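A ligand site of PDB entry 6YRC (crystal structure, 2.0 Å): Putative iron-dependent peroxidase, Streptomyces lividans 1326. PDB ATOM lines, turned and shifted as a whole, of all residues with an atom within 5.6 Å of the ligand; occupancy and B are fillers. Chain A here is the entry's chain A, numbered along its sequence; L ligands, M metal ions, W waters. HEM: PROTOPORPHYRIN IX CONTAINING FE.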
ATOM      1  N   ASP A 146      -0.297 -27.318  -4.618  1.00  0.00           N
ATOM      2  CA  ASP A 146      -0.083 -25.997  -3.990  1.00  0.00           C
ATOM      3  C   ASP A 146      -0.883 -24.969  -4.807  1.00  0.00           C
ATOM      4  O   ASP A 146      -1.644 -25.358  -5.749  1.00  0.00           O
ATOM      5  CB  ASP A 146       1.410 -25.711  -3.839  1.00  0.00           C
ATOM      6  CG  ASP A 146       2.177 -25.679  -5.142  1.00  0.00           C
ATOM      7  OD1 ASP A 146       1.574 -25.330  -6.176  1.00  0.00           O
ATOM      8  OD2 ASP A 146       3.385 -26.027  -5.100  1.00  0.00           O
ATOM      9  N   LEU A 148       0.073 -22.867  -6.879  1.00  0.00           N
ATOM     10  CA  LEU A 148       0.546 -22.782  -8.292  1.00  0.00           C
ATOM     11  C   LEU A 148      -0.062 -23.895  -9.162  1.00  0.00           C
ATOM     12  O   LEU A 148       0.184 -23.880 -10.392  1.00  0.00           O
ATOM     13  CB  LEU A 148       2.073 -22.791  -8.327  1.00  0.00           C
ATOM     14  CG  LEU A 148       2.779 -21.650  -7.587  1.00  0.00           C
ATOM     15  CD1 LEU A 148       4.282 -21.697  -7.811  1.00  0.00           C
ATOM     16  CD2 LEU A 148       2.207 -20.284  -7.965  1.00  0.00           C
ATOM     17  N   PHE A 150       0.552 -27.134  -8.919  1.00  0.00           N
ATOM     18  CA  PHE A 150       1.476 -28.298  -9.015  1.00  0.00           C
ATOM     19  C   PHE A 150       1.371 -29.151  -7.761  1.00  0.00           C
ATOM     20  O   PHE A 150       1.157 -28.618  -6.625  1.00  0.00           O
ATOM     21  CB  PHE A 150       2.906 -27.840  -9.264  1.00  0.00           C
ATOM     22  CG  PHE A 150       3.175 -27.403 -10.675  1.00  0.00           C
ATOM     23  CD1 PHE A 150       2.593 -26.255 -11.191  1.00  0.00           C
ATOM     24  CD2 PHE A 150       3.978 -28.167 -11.510  1.00  0.00           C
ATOM     25  CE1 PHE A 150       2.851 -25.873 -12.491  1.00  0.00           C
ATOM     26  CE2 PHE A 150       4.197 -27.795 -12.817  1.00  0.00           C
ATOM     27  CZ  PHE A 150       3.645 -26.635 -13.300  1.00  0.00           C
ATOM     28  N   VAL A 151       1.593 -30.462  -7.943  1.00  0.00           N
ATOM     29  CA  VAL A 151       1.774 -31.426  -6.820  1.00  0.00           C
ATOM     30  C   VAL A 151       3.002 -31.009  -6.017  1.00  0.00           C
ATOM     31  O   VAL A 151       4.078 -30.723  -6.630  1.00  0.00           O
ATOM     32  CB  VAL A 151       1.906 -32.885  -7.285  1.00  0.00           C
ATOM     33  CG1 VAL A 151       2.088 -33.792  -6.088  1.00  0.00           C
ATOM     34  CG2 VAL A 151       0.710 -33.330  -8.127  1.00  0.00           C
ATOM     35  N   ASP A 152       2.869 -31.057  -4.700  1.00  0.00           N
ATOM     36  CA  ASP A 152       3.900 -30.509  -3.779  1.00  0.00           C
ATOM     37  C   ASP A 152       4.191 -31.555  -2.696  1.00  0.00           C
ATOM     38  O   ASP A 152       3.295 -31.842  -1.890  1.00  0.00           O
ATOM     39  CB  ASP A 152       3.399 -29.163  -3.272  1.00  0.00           C
ATOM     40  CG  ASP A 152       4.508 -28.317  -2.688  1.00  0.00           C
ATOM     41  OD1 ASP A 152       5.299 -28.898  -1.901  1.00  0.00           O
ATOM     42  OD2 ASP A 152       4.519 -27.082  -2.976  1.00  0.00           O
ATOM     43  N   GLY A 153       5.415 -32.094  -2.670  1.00  0.00           N
ATOM     44  CA  GLY A 153       5.836 -33.119  -1.698  1.00  0.00           C
ATOM     45  C   GLY A 153       6.413 -34.368  -2.363  1.00  0.00           C
ATOM     46  O   GLY A 153       7.025 -35.145  -1.655  1.00  0.00           O
ATOM     47  N   THR A 154       6.259 -34.518  -3.679  1.00  0.00           N
ATOM     48  CA  THR A 154       6.586 -35.758  -4.451  1.00  0.00           C
ATOM     49  C   THR A 154       7.967 -36.296  -4.066  1.00  0.00           C
ATOM     50  O   THR A 154       8.060 -37.474  -3.698  1.00  0.00           O
ATOM     51  CB  THR A 154       6.507 -35.483  -5.953  1.00  0.00           C
ATOM     52  OG1 THR A 154       5.254 -34.830  -6.167  1.00  0.00           O
ATOM     53  CG2 THR A 154       6.629 -36.733  -6.807  1.00  0.00           C
ATOM     54  N   GLU A 155       9.016 -35.461  -4.108  1.00  0.00           N
ATOM     55  CA  GLU A 155      10.408 -35.942  -3.970  1.00  0.00           C
ATOM     56  C   GLU A 155      10.873 -35.861  -2.514  1.00  0.00           C
ATOM     57  O   GLU A 155      12.094 -36.087  -2.261  1.00  0.00           O
ATOM     58  CB  GLU A 155      11.323 -35.193  -4.947  1.00  0.00           C
ATOM     59  CG  GLU A 155      11.118 -35.606  -6.384  1.00  0.00           C
ATOM     60  CD  GLU A 155      11.212 -37.111  -6.612  1.00  0.00           C
ATOM     61  OE1 GLU A 155      12.320 -37.612  -6.578  1.00  0.00           O
ATOM     62  OE2 GLU A 155      10.170 -37.775  -6.696  1.00  0.00           O
ATOM     63  N   ASN A 156       9.990 -35.578  -1.553  1.00  0.00           N
ATOM     64  CA  ASN A 156      10.383 -35.654  -0.110  1.00  0.00           C
ATOM     65  C   ASN A 156      10.999 -37.014   0.179  1.00  0.00           C
ATOM     66  O   ASN A 156      10.499 -38.049  -0.271  1.00  0.00           O
ATOM     67  CB  ASN A 156       9.190 -35.447   0.816  1.00  0.00           C
ATOM     68  CG  ASN A 156       9.041 -34.001   1.246  1.00  0.00           C
ATOM     69  OD1 ASN A 156      10.042 -33.309   1.396  1.00  0.00           O
ATOM     70  ND2 ASN A 156       7.808 -33.542   1.408  1.00  0.00           N
ATOM     71  N   GLN A 184       9.179 -19.923   5.788  1.00  0.00           N
ATOM     72  CA  GLN A 184       8.957 -18.708   4.979  1.00  0.00           C
ATOM     73  C   GLN A 184       7.496 -18.729   4.550  1.00  0.00           C
ATOM     74  O   GLN A 184       7.083 -19.710   3.882  1.00  0.00           O
ATOM     75  CB  GLN A 184       9.830 -18.666   3.738  1.00  0.00           C
ATOM     76  CG  GLN A 184      11.327 -18.646   3.999  1.00  0.00           C
ATOM     77  CD  GLN A 184      12.042 -18.599   2.676  1.00  0.00           C
ATOM     78  OE1 GLN A 184      12.015 -19.579   1.923  1.00  0.00           O
ATOM     79  NE2 GLN A 184      12.570 -17.428   2.333  1.00  0.00           N
ATOM     80  N   TYR A 186       5.039 -17.495   1.889  1.00  0.00           N
ATOM     81  CA  TYR A 186       5.082 -16.962   0.504  1.00  0.00           C
ATOM     82  C   TYR A 186       3.668 -16.559   0.106  1.00  0.00           C
ATOM     83  O   TYR A 186       2.682 -17.349   0.296  1.00  0.00           O
ATOM     84  CB  TYR A 186       5.670 -17.942  -0.522  1.00  0.00           C
ATOM     85  CG  TYR A 186       7.168 -18.140  -0.500  1.00  0.00           C
ATOM     86  CD1 TYR A 186       8.013 -17.342  -1.255  1.00  0.00           C
ATOM     87  CD2 TYR A 186       7.744 -19.112   0.308  1.00  0.00           C
ATOM     88  CE1 TYR A 186       9.395 -17.538  -1.238  1.00  0.00           C
ATOM     89  CE2 TYR A 186       9.118 -19.301   0.360  1.00  0.00           C
ATOM     90  CZ  TYR A 186       9.945 -18.500  -0.417  1.00  0.00           C
ATOM     91  OH  TYR A 186      11.298 -18.737  -0.402  1.00  0.00           O
ATOM     92  N   HIS A 188       1.700 -15.601  -3.616  1.00  0.00           N
ATOM     93  CA  HIS A 188       1.908 -15.792  -5.070  1.00  0.00           C
ATOM     94  C   HIS A 188       1.199 -14.681  -5.857  1.00  0.00           C
ATOM     95  O   HIS A 188       0.101 -14.296  -5.476  1.00  0.00           O
ATOM     96  CB  HIS A 188       1.437 -17.172  -5.488  1.00  0.00           C
ATOM     97  CG  HIS A 188       2.203 -18.279  -4.830  1.00  0.00           C
ATOM     98  ND1 HIS A 188       3.502 -18.581  -5.186  1.00  0.00           N
ATOM     99  CD2 HIS A 188       1.854 -19.148  -3.875  1.00  0.00           C
ATOM    100  CE1 HIS A 188       3.905 -19.598  -4.447  1.00  0.00           C
ATOM    101  NE2 HIS A 188       2.916 -19.991  -3.655  1.00  0.00           N
ATOM    102  N   ILE A 205       8.828 -24.718 -12.911  1.00  0.00           N
ATOM    103  CA  ILE A 205       8.852 -25.691 -11.762  1.00  0.00           C
ATOM    104  C   ILE A 205       9.908 -26.773 -12.047  1.00  0.00           C
ATOM    105  O   ILE A 205      10.716 -27.055 -11.114  1.00  0.00           O
ATOM    106  CB  ILE A 205       7.458 -26.295 -11.540  1.00  0.00           C
ATOM    107  CG1 ILE A 205       6.420 -25.223 -11.180  1.00  0.00           C
ATOM    108  CG2 ILE A 205       7.495 -27.403 -10.479  1.00  0.00           C
ATOM    109  CD1 ILE A 205       6.619 -24.578  -9.829  1.00  0.00           C
ATOM    110  N   ARG A 207       8.832 -29.814 -13.546  1.00  0.00           N
ATOM    111  CA  ARG A 207       8.018 -31.061 -13.635  1.00  0.00           C
ATOM    112  C   ARG A 207       6.794 -30.786 -14.495  1.00  0.00           C
ATOM    113  O   ARG A 207       6.435 -29.609 -14.591  1.00  0.00           O
ATOM    114  CB  ARG A 207       7.586 -31.574 -12.251  1.00  0.00           C
ATOM    115  CG  ARG A 207       8.667 -31.577 -11.184  1.00  0.00           C
ATOM    116  CD  ARG A 207       8.185 -32.168  -9.882  1.00  0.00           C
ATOM    117  NE  ARG A 207       7.839 -33.577 -10.011  1.00  0.00           N
ATOM    118  CZ  ARG A 207       8.670 -34.602  -9.816  1.00  0.00           C
ATOM    119  NH1 ARG A 207       9.929 -34.368  -9.455  1.00  0.00           N
ATOM    120  NH2 ARG A 207       8.256 -35.839 -10.000  1.00  0.00           N
ATOM    121  N   ASP A 212       2.854 -34.767 -12.995  1.00  0.00           N
ATOM    122  CA  ASP A 212       3.911 -34.631 -11.950  1.00  0.00           C
ATOM    123  C   ASP A 212       5.149 -35.474 -12.307  1.00  0.00           C
ATOM    124  O   ASP A 212       5.829 -35.979 -11.389  1.00  0.00           O
ATOM    125  CB  ASP A 212       3.355 -35.029 -10.593  1.00  0.00           C
ATOM    126  CG  ASP A 212       4.246 -34.609  -9.440  1.00  0.00           C
ATOM    127  OD1 ASP A 212       5.097 -33.673  -9.626  1.00  0.00           O
ATOM    128  OD2 ASP A 212       4.071 -35.224  -8.356  1.00  0.00           O
ATOM    129  N   GLU A 214       8.990 -35.552 -13.602  1.00  0.00           N
ATOM    130  CA  GLU A 214      10.156 -34.636 -13.679  1.00  0.00           C
ATOM    131  C   GLU A 214      10.556 -34.432 -15.161  1.00  0.00           C
ATOM    132  O   GLU A 214      10.523 -35.394 -15.925  1.00  0.00           O
ATOM    133  CB  GLU A 214      11.302 -35.168 -12.815  1.00  0.00           C
ATOM    134  CG  GLU A 214      12.421 -34.166 -12.740  1.00  0.00           C
ATOM    135  CD  GLU A 214      13.510 -34.520 -11.754  1.00  0.00           C
ATOM    136  OE1 GLU A 214      13.422 -35.580 -11.118  1.00  0.00           O
ATOM    137  OE2 GLU A 214      14.416 -33.711 -11.628  1.00  0.00           O
ATOM    138  N   HIS A 225      12.848 -24.456 -10.559  1.00  0.00           N
ATOM    139  CA  HIS A 225      12.814 -24.711  -9.099  1.00  0.00           C
ATOM    140  C   HIS A 225      13.493 -26.059  -8.750  1.00  0.00           C
ATOM    141  O   HIS A 225      14.355 -26.104  -7.814  1.00  0.00           O
ATOM    142  CB  HIS A 225      11.363 -24.683  -8.645  1.00  0.00           C
ATOM    143  CG  HIS A 225      11.253 -24.791  -7.173  1.00  0.00           C
ATOM    144  ND1 HIS A 225      11.985 -23.956  -6.329  1.00  0.00           N
ATOM    145  CD2 HIS A 225      10.495 -25.593  -6.379  1.00  0.00           C
ATOM    146  CE1 HIS A 225      11.691 -24.256  -5.060  1.00  0.00           C
ATOM    147  NE2 HIS A 225      10.779 -25.266  -5.067  1.00  0.00           N
ATOM    148  N   VAL A 226      13.080 -27.140  -9.415  1.00  0.00           N
ATOM    149  CA  VAL A 226      13.616 -28.502  -9.163  1.00  0.00           C
ATOM    150  C   VAL A 226      15.118 -28.542  -9.441  1.00  0.00           C
ATOM    151  O   VAL A 226      15.816 -29.120  -8.604  1.00  0.00           O
ATOM    152  CB  VAL A 226      12.843 -29.577  -9.938  1.00  0.00           C
ATOM    153  CG1 VAL A 226      13.604 -30.908  -9.967  1.00  0.00           C
ATOM    154  CG2 VAL A 226      11.465 -29.771  -9.312  1.00  0.00           C
ATOM    155  N   THR A 229      16.923 -26.614  -6.461  1.00  0.00           N
ATOM    156  CA  THR A 229      16.721 -27.225  -5.116  1.00  0.00           C
ATOM    157  C   THR A 229      17.154 -28.693  -5.109  1.00  0.00           C
ATOM    158  O   THR A 229      17.043 -29.307  -4.032  1.00  0.00           O
ATOM    159  CB  THR A 229      15.293 -27.050  -4.591  1.00  0.00           C
ATOM    160  OG1 THR A 229      14.365 -27.681  -5.463  1.00  0.00           O
ATOM    161  CG2 THR A 229      14.911 -25.595  -4.421  1.00  0.00           C
ATOM    162  N   SER A 230      17.681 -29.186  -6.237  1.00  0.00           N
ATOM    163  CA  SER A 230      18.402 -30.479  -6.327  1.00  0.00           C
ATOM    164  C   SER A 230      19.894 -30.244  -6.009  1.00  0.00           C
ATOM    165  O   SER A 230      20.571 -29.511  -6.748  1.00  0.00           O
ATOM    166  CB  SER A 230      18.193 -31.093  -7.683  1.00  0.00           C
ATOM    167  OG  SER A 230      16.837 -31.479  -7.833  1.00  0.00           O
ATOM    168  N   ILE A 241      16.009 -32.327   2.253  1.00  0.00           N
ATOM    169  CA  ILE A 241      15.241 -31.746   3.380  1.00  0.00           C
ATOM    170  C   ILE A 241      13.855 -32.375   3.335  1.00  0.00           C
ATOM    171  O   ILE A 241      13.519 -32.968   2.271  1.00  0.00           O
ATOM    172  CB  ILE A 241      15.220 -30.223   3.258  1.00  0.00           C
ATOM    173  CG1 ILE A 241      14.401 -29.740   2.064  1.00  0.00           C
ATOM    174  CG2 ILE A 241      16.653 -29.699   3.212  1.00  0.00           C
ATOM    175  CD1 ILE A 241      14.120 -28.239   2.104  1.00  0.00           C
ATOM    176  N   ARG A 243      10.023 -31.314   3.538  1.00  0.00           N
ATOM    177  CA  ARG A 243       9.082 -30.172   3.434  1.00  0.00           C
ATOM    178  C   ARG A 243       7.675 -30.620   3.841  1.00  0.00           C
ATOM    179  O   ARG A 243       7.302 -31.781   3.570  1.00  0.00           O
ATOM    180  CB  ARG A 243       9.050 -29.655   2.007  1.00  0.00           C
ATOM    181  CG  ARG A 243      10.314 -28.942   1.567  1.00  0.00           C
ATOM    182  CD  ARG A 243      10.292 -28.781   0.037  1.00  0.00           C
ATOM    183  NE  ARG A 243      10.441 -30.081  -0.609  1.00  0.00           N
ATOM    184  CZ  ARG A 243       9.595 -30.620  -1.477  1.00  0.00           C
ATOM    185  NH1 ARG A 243       8.512 -29.958  -1.856  1.00  0.00           N
ATOM    186  NH2 ARG A 243       9.856 -31.825  -1.996  1.00  0.00           N
ATOM    187  N   ASN A 245       4.916 -28.223   2.913  1.00  0.00           N
ATOM    188  CA  ASN A 245       4.377 -26.925   2.422  1.00  0.00           C
ATOM    189  C   ASN A 245       2.855 -26.955   2.566  1.00  0.00           C
ATOM    190  O   ASN A 245       2.270 -28.002   2.259  1.00  0.00           O
ATOM    191  CB  ASN A 245       4.715 -26.675   0.953  1.00  0.00           C
ATOM    192  CG  ASN A 245       6.155 -26.278   0.741  1.00  0.00           C
ATOM    193  OD1 ASN A 245       6.896 -26.181   1.717  1.00  0.00           O
ATOM    194  ND2 ASN A 245       6.554 -26.102  -0.514  1.00  0.00           N
ATOM    195  N   THR A 258       1.806 -20.007  -0.173  1.00  0.00           N
ATOM    196  CA  THR A 258       2.429 -21.306   0.221  1.00  0.00           C
ATOM    197  C   THR A 258       3.144 -21.017   1.534  1.00  0.00           C
ATOM    198  O   THR A 258       4.037 -20.134   1.554  1.00  0.00           O
ATOM    199  CB  THR A 258       3.397 -21.846  -0.842  1.00  0.00           C
ATOM    200  OG1 THR A 258       2.683 -22.108  -2.050  1.00  0.00           O
ATOM    201  CG2 THR A 258       4.123 -23.099  -0.396  1.00  0.00           C
ATOM    202  N   PHE A 260       5.880 -22.331   3.457  1.00  0.00           N
ATOM    203  CA  PHE A 260       7.020 -23.249   3.324  1.00  0.00           C
ATOM    204  C   PHE A 260       7.526 -23.560   4.728  1.00  0.00           C
ATOM    205  O   PHE A 260       7.700 -22.612   5.522  1.00  0.00           O
ATOM    206  CB  PHE A 260       8.163 -22.619   2.519  1.00  0.00           C
ATOM    207  CG  PHE A 260       9.428 -23.417   2.615  1.00  0.00           C
ATOM    208  CD1 PHE A 260       9.630 -24.523   1.792  1.00  0.00           C
ATOM    209  CD2 PHE A 260      10.408 -23.090   3.534  1.00  0.00           C
ATOM    210  CE1 PHE A 260      10.811 -25.261   1.886  1.00  0.00           C
ATOM    211  CE2 PHE A 260      11.587 -23.820   3.611  1.00  0.00           C
ATOM    212  CZ  PHE A 260      11.771 -24.924   2.804  1.00  0.00           C
ATOM    213  N   THR A 270      19.424 -26.540   3.970  1.00  0.00           N
ATOM    214  CA  THR A 270      18.303 -25.626   3.636  1.00  0.00           C
ATOM    215  C   THR A 270      18.850 -24.290   3.119  1.00  0.00           C
ATOM    216  O   THR A 270      18.302 -23.747   2.127  1.00  0.00           O
ATOM    217  CB  THR A 270      17.347 -25.453   4.823  1.00  0.00           C
ATOM    218  OG1 THR A 270      17.112 -26.716   5.437  1.00  0.00           O
ATOM    219  CG2 THR A 270      16.025 -24.883   4.376  1.00  0.00           C
ATOM    220  N   MET A 273      20.164 -24.465  -0.470  1.00  0.00           N
ATOM    221  CA  MET A 273      18.987 -24.379  -1.380  1.00  0.00           C
ATOM    222  C   MET A 273      18.536 -22.910  -1.491  1.00  0.00           C
ATOM    223  O   MET A 273      18.408 -22.419  -2.606  1.00  0.00           O
ATOM    224  CB  MET A 273      17.872 -25.277  -0.862  1.00  0.00           C
ATOM    225  CG  MET A 273      18.222 -26.735  -0.961  1.00  0.00           C
ATOM    226  SD  MET A 273      16.988 -27.823  -0.239  1.00  0.00           S
ATOM    227  CE  MET A 273      17.564 -29.426  -0.822  1.00  0.00           C
ATOM    228  N   LEU A 274      18.304 -22.204  -0.377  1.00  0.00           N
ATOM    229  CA  LEU A 274      17.835 -20.793  -0.410  1.00  0.00           C
ATOM    230  C   LEU A 274      18.831 -19.927  -1.203  1.00  0.00           C
ATOM    231  O   LEU A 274      18.367 -19.063  -1.973  1.00  0.00           O
ATOM    232  CB  LEU A 274      17.660 -20.285   1.013  1.00  0.00           C
ATOM    233  CG  LEU A 274      16.436 -20.847   1.748  1.00  0.00           C
ATOM    234  CD1 LEU A 274      16.457 -20.479   3.217  1.00  0.00           C
ATOM    235  CD2 LEU A 274      15.152 -20.362   1.099  1.00  0.00           C
ATOM    236  N   MET A 277      18.423 -20.421  -4.844  1.00  0.00           N
ATOM    237  CA  MET A 277      17.124 -19.844  -5.253  1.00  0.00           C
ATOM    238  C   MET A 277      17.227 -18.318  -5.376  1.00  0.00           C
ATOM    239  O   MET A 277      16.817 -17.786  -6.399  1.00  0.00           O
ATOM    240  CB  MET A 277      16.052 -20.228  -4.236  1.00  0.00           C
ATOM    241  CG  MET A 277      15.659 -21.683  -4.261  1.00  0.00           C
ATOM    242  SD  MET A 277      14.407 -22.077  -3.015  1.00  0.00           S
ATOM    243  CE  MET A 277      13.058 -20.987  -3.448  1.00  0.00           C
ATOM    244  N   ILE A 289      10.572 -19.600  -9.872  1.00  0.00           N
ATOM    245  CA  ILE A 289       9.386 -19.668  -8.977  1.00  0.00           C
ATOM    246  C   ILE A 289       9.284 -18.356  -8.194  1.00  0.00           C
ATOM    247  O   ILE A 289       8.171 -17.962  -7.864  1.00  0.00           O
ATOM    248  CB  ILE A 289       9.394 -20.897  -8.050  1.00  0.00           C
ATOM    249  CG1 ILE A 289       7.973 -21.387  -7.760  1.00  0.00           C
ATOM    250  CG2 ILE A 289      10.181 -20.644  -6.747  1.00  0.00           C
ATOM    251  CD1 ILE A 289       7.908 -22.614  -6.874  1.00  0.00           C
ATOM    252  N   LEU A 290      10.409 -17.711  -7.913  1.00  0.00           N
ATOM    253  CA  LEU A 290      10.442 -16.438  -7.154  1.00  0.00           C
ATOM    254  C   LEU A 290       9.892 -15.283  -7.990  1.00  0.00           C
ATOM    255  O   LEU A 290       9.503 -14.281  -7.390  1.00  0.00           O
ATOM    256  CB  LEU A 290      11.869 -16.136  -6.689  1.00  0.00           C
ATOM    257  CG  LEU A 290      12.393 -17.127  -5.658  1.00  0.00           C
ATOM    258  CD1 LEU A 290      13.837 -16.780  -5.263  1.00  0.00           C
ATOM    259  CD2 LEU A 290      11.486 -17.157  -4.451  1.00  0.00           C
ATOM    260  N   SER A 293       6.440 -15.554  -6.629  1.00  0.00           N
ATOM    261  CA  SER A 293       6.440 -15.949  -5.211  1.00  0.00           C
ATOM    262  C   SER A 293       7.242 -14.920  -4.402  1.00  0.00           C
ATOM    263  O   SER A 293       8.461 -14.783  -4.677  1.00  0.00           O
ATOM    264  CB  SER A 293       6.953 -17.365  -5.004  1.00  0.00           C
ATOM    265  OG  SER A 293       6.352 -18.304  -5.879  1.00  0.00           O
HETATM  266  CHA HEM L   1      10.187 -29.367  -4.989  1.00  0.00           C
HETATM  267  CHB HEM L   1       6.790 -25.944  -4.722  1.00  0.00           C
HETATM  268  CHC HEM L   1       9.708 -23.260  -1.923  1.00  0.00           C
HETATM  269  CHD HEM L   1      12.825 -26.986  -1.670  1.00  0.00           C
HETATM  270  C1A HEM L   1       9.036 -28.621  -5.170  1.00  0.00           C
HETATM  271  C2A HEM L   1       8.012 -28.982  -6.103  1.00  0.00           C
HETATM  272  C3A HEM L   1       7.043 -28.015  -6.038  1.00  0.00           C
HETATM  273  C4A HEM L   1       7.453 -27.082  -5.044  1.00  0.00           C
HETATM  274  CMA HEM L   1       5.752 -27.965  -6.806  1.00  0.00           C
HETATM  275  CAA HEM L   1       8.056 -30.218  -6.994  1.00  0.00           C
HETATM  276  CBA HEM L   1       7.405 -31.433  -6.354  1.00  0.00           C
HETATM  277  CGA HEM L   1       8.167 -31.924  -5.150  1.00  0.00           C
HETATM  278  O1A HEM L   1       7.798 -31.534  -4.013  1.00  0.00           O
HETATM  279  O2A HEM L   1       9.120 -32.734  -5.288  1.00  0.00           O
HETATM  280  C1B HEM L   1       7.282 -24.915  -3.936  1.00  0.00           C
HETATM  281  C2B HEM L   1       6.569 -23.673  -3.705  1.00  0.00           C
HETATM  282  C3B HEM L   1       7.356 -22.923  -2.919  1.00  0.00           C
HETATM  283  C4B HEM L   1       8.625 -23.679  -2.680  1.00  0.00           C
HETATM  284  CMB HEM L   1       5.208 -23.254  -4.190  1.00  0.00           C
HETATM  285  CAB HEM L   1       7.001 -21.534  -2.578  1.00  0.00           C
HETATM  286  CBB HEM L   1       7.933 -20.590  -2.682  1.00  0.00           C
HETATM  287  C1C HEM L   1      10.829 -24.033  -1.594  1.00  0.00           C
HETATM  288  C2C HEM L   1      11.910 -23.615  -0.763  1.00  0.00           C
HETATM  289  C3C HEM L   1      12.833 -24.670  -0.721  1.00  0.00           C
HETATM  290  C4C HEM L   1      12.253 -25.761  -1.492  1.00  0.00           C
HETATM  291  CMC HEM L   1      12.022 -22.249  -0.062  1.00  0.00           C
HETATM  292  CAC HEM L   1      14.090 -24.814   0.032  1.00  0.00           C
HETATM  293  CBC HEM L   1      14.500 -23.937   0.915  1.00  0.00           C
HETATM  294  C1D HEM L   1      12.304 -27.931  -2.576  1.00  0.00           C
HETATM  295  C2D HEM L   1      13.003 -29.212  -2.765  1.00  0.00           C
HETATM  296  C3D HEM L   1      12.266 -29.880  -3.679  1.00  0.00           C
HETATM  297  C4D HEM L   1      11.136 -28.976  -4.054  1.00  0.00           C
HETATM  298  CMD HEM L   1      14.235 -29.732  -2.044  1.00  0.00           C
HETATM  299  CAD HEM L   1      12.596 -31.255  -4.218  1.00  0.00           C
HETATM  300  CBD HEM L   1      13.501 -31.113  -5.460  1.00  0.00           C
HETATM  301  CGD HEM L   1      13.972 -32.501  -5.932  1.00  0.00           C
HETATM  302  O1D HEM L   1      14.926 -33.064  -5.348  1.00  0.00           O
HETATM  303  O2D HEM L   1      13.427 -33.096  -6.899  1.00  0.00           O
HETATM  304  NA  HEM L   1       8.675 -27.437  -4.536  1.00  0.00           N
HETATM  305  NB  HEM L   1       8.478 -24.852  -3.312  1.00  0.00           N
HETATM  306  NC  HEM L   1      11.038 -25.336  -2.022  1.00  0.00           N
HETATM  307  ND  HEM L   1      11.161 -27.830  -3.346  1.00  0.00           N
HETATM  308 FE   HEM L   1       9.929 -26.316  -3.474  1.00  0.00          FE
HETATM  309 MG    MG M   1      16.301 -35.863  -8.114  1.00  0.00          MG
HETATM  310  O   HOH W   1      16.956 -34.513  -6.663  1.00  0.00           O
HETATM  311  O   HOH W   2      16.225 -31.920  -3.261  1.00  0.00           O
HETATM  312  O   HOH W   3      10.827 -32.462  -7.477  1.00  0.00           O
HETATM  313  O   HOH W   4      14.137 -35.366  -8.031  1.00  0.00           O
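A ring nitrogen (NE2) of His 225 is bound to an iron atom (FE) of the ligand (2.1 Å). An oxygen (O1A) of the ligand is in hydrogen-bond range of the backbone NH (N) of Gly 153. An oxygen (O2A) of the ligand sits at hydrogen-bond distance from the backbone NH (N) of Glu 155 (3.0 Å). The backbone NH (N) of Thr 154 is in hydrogen-bond range of an oxygen (O1A) of the ligand. An oxygen (O1A) of the ligand is in salt-bridge range of the guanidinium group (NH1) of Arg 243, at 2.8 Å.
O of Arg 243 sits at hydrogen-bond distance from ND2 of Asn 156, at 2.8 Å. The side-chain carboxylate (OD1) of Asp 152 is in salt-bridge range of the guanidinium group (NH1) of Arg 243, 3.4 Å away. The side-chain hydroxyl of Ser 230 is in hydrogen-bond range of the backbone carbonyl oxygen of Val 226, at 2.7 Å. OD1 of Asp 146 lies within hydrogen-bond range of N of Phe 150, 3.4 Å away. The side-chain hydroxyl (OG1) of Thr 229 lies within hydrogen-bond range of the backbone carbonyl oxygen (O) of His 225. N of His 225 sits at hydrogen-bond distance from O of Ile 205 (3.4 Å). OD2 of Asp 152 lies close to OD2 of Asp 146. The backbone carbonyl oxygen of Ile 289 lies within hydrogen-bond range of the side-chain hydroxyl of Ser 293 (2.7 Å).
Merely in contact with the ligand: Asp 146 (3.4 Å), Phe 150 (3.8 Å), Val 151 (3.2 Å), Asp 152 (3.1 Å), Gln 184 (3.3 Å), Tyr 186 (3.3 Å), His 188 (3.9 Å), Arg 207 (3.5 Å), Val 226 (3.8 Å), Thr 229 (3.4 Å), Ser 230 (3.5 Å), Asn 245 (3.6 Å), Thr 258 (3.5 Å), Phe 260 (3.3 Å), Thr 270 (3.9 Å), Met 273 (3.6 Å), Leu 274 (3.6 Å), Met 277 (3.7 Å) and Ile 289 (3.6 Å). Within 4 Å of the ligand: Asp 146, Phe 150, Val 151, Asp 152, Gly 153, Thr 154, Glu 155, Gln 184, Tyr 186, His 188, Arg 207, His 225, Val 226, Thr 229, Ser 230, Arg 243, Asn 245, Thr 258, Phe 260, Thr 270, Met 273, Leu 274, Met 277 and Ile 289. The nearest printed residue that does not touch the ligand is Ile 241 (4.003 Å).
Water W4 lies within hydrogen-bond range of an oxygen (O2D) of the ligand, the side-chain carboxylate (OE1) of Glu 214 and the side-chain carboxylate (OE1) of Glu 155. Water W2 lies within hydrogen-bond range of an oxygen (O1D) of the ligand and the backbone carbonyl oxygen (O) of Thr 229. Water W3 lies within hydrogen-bond range of O2D of the ligand (2.7 Å) and NH1 of Arg 207 (2.9 Å). Water W1 lies within hydrogen-bond range of an oxygen (O1D) of the ligand (2.8 Å) and the side-chain hydroxyl (OG) of Ser 230 (3.3 Å).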
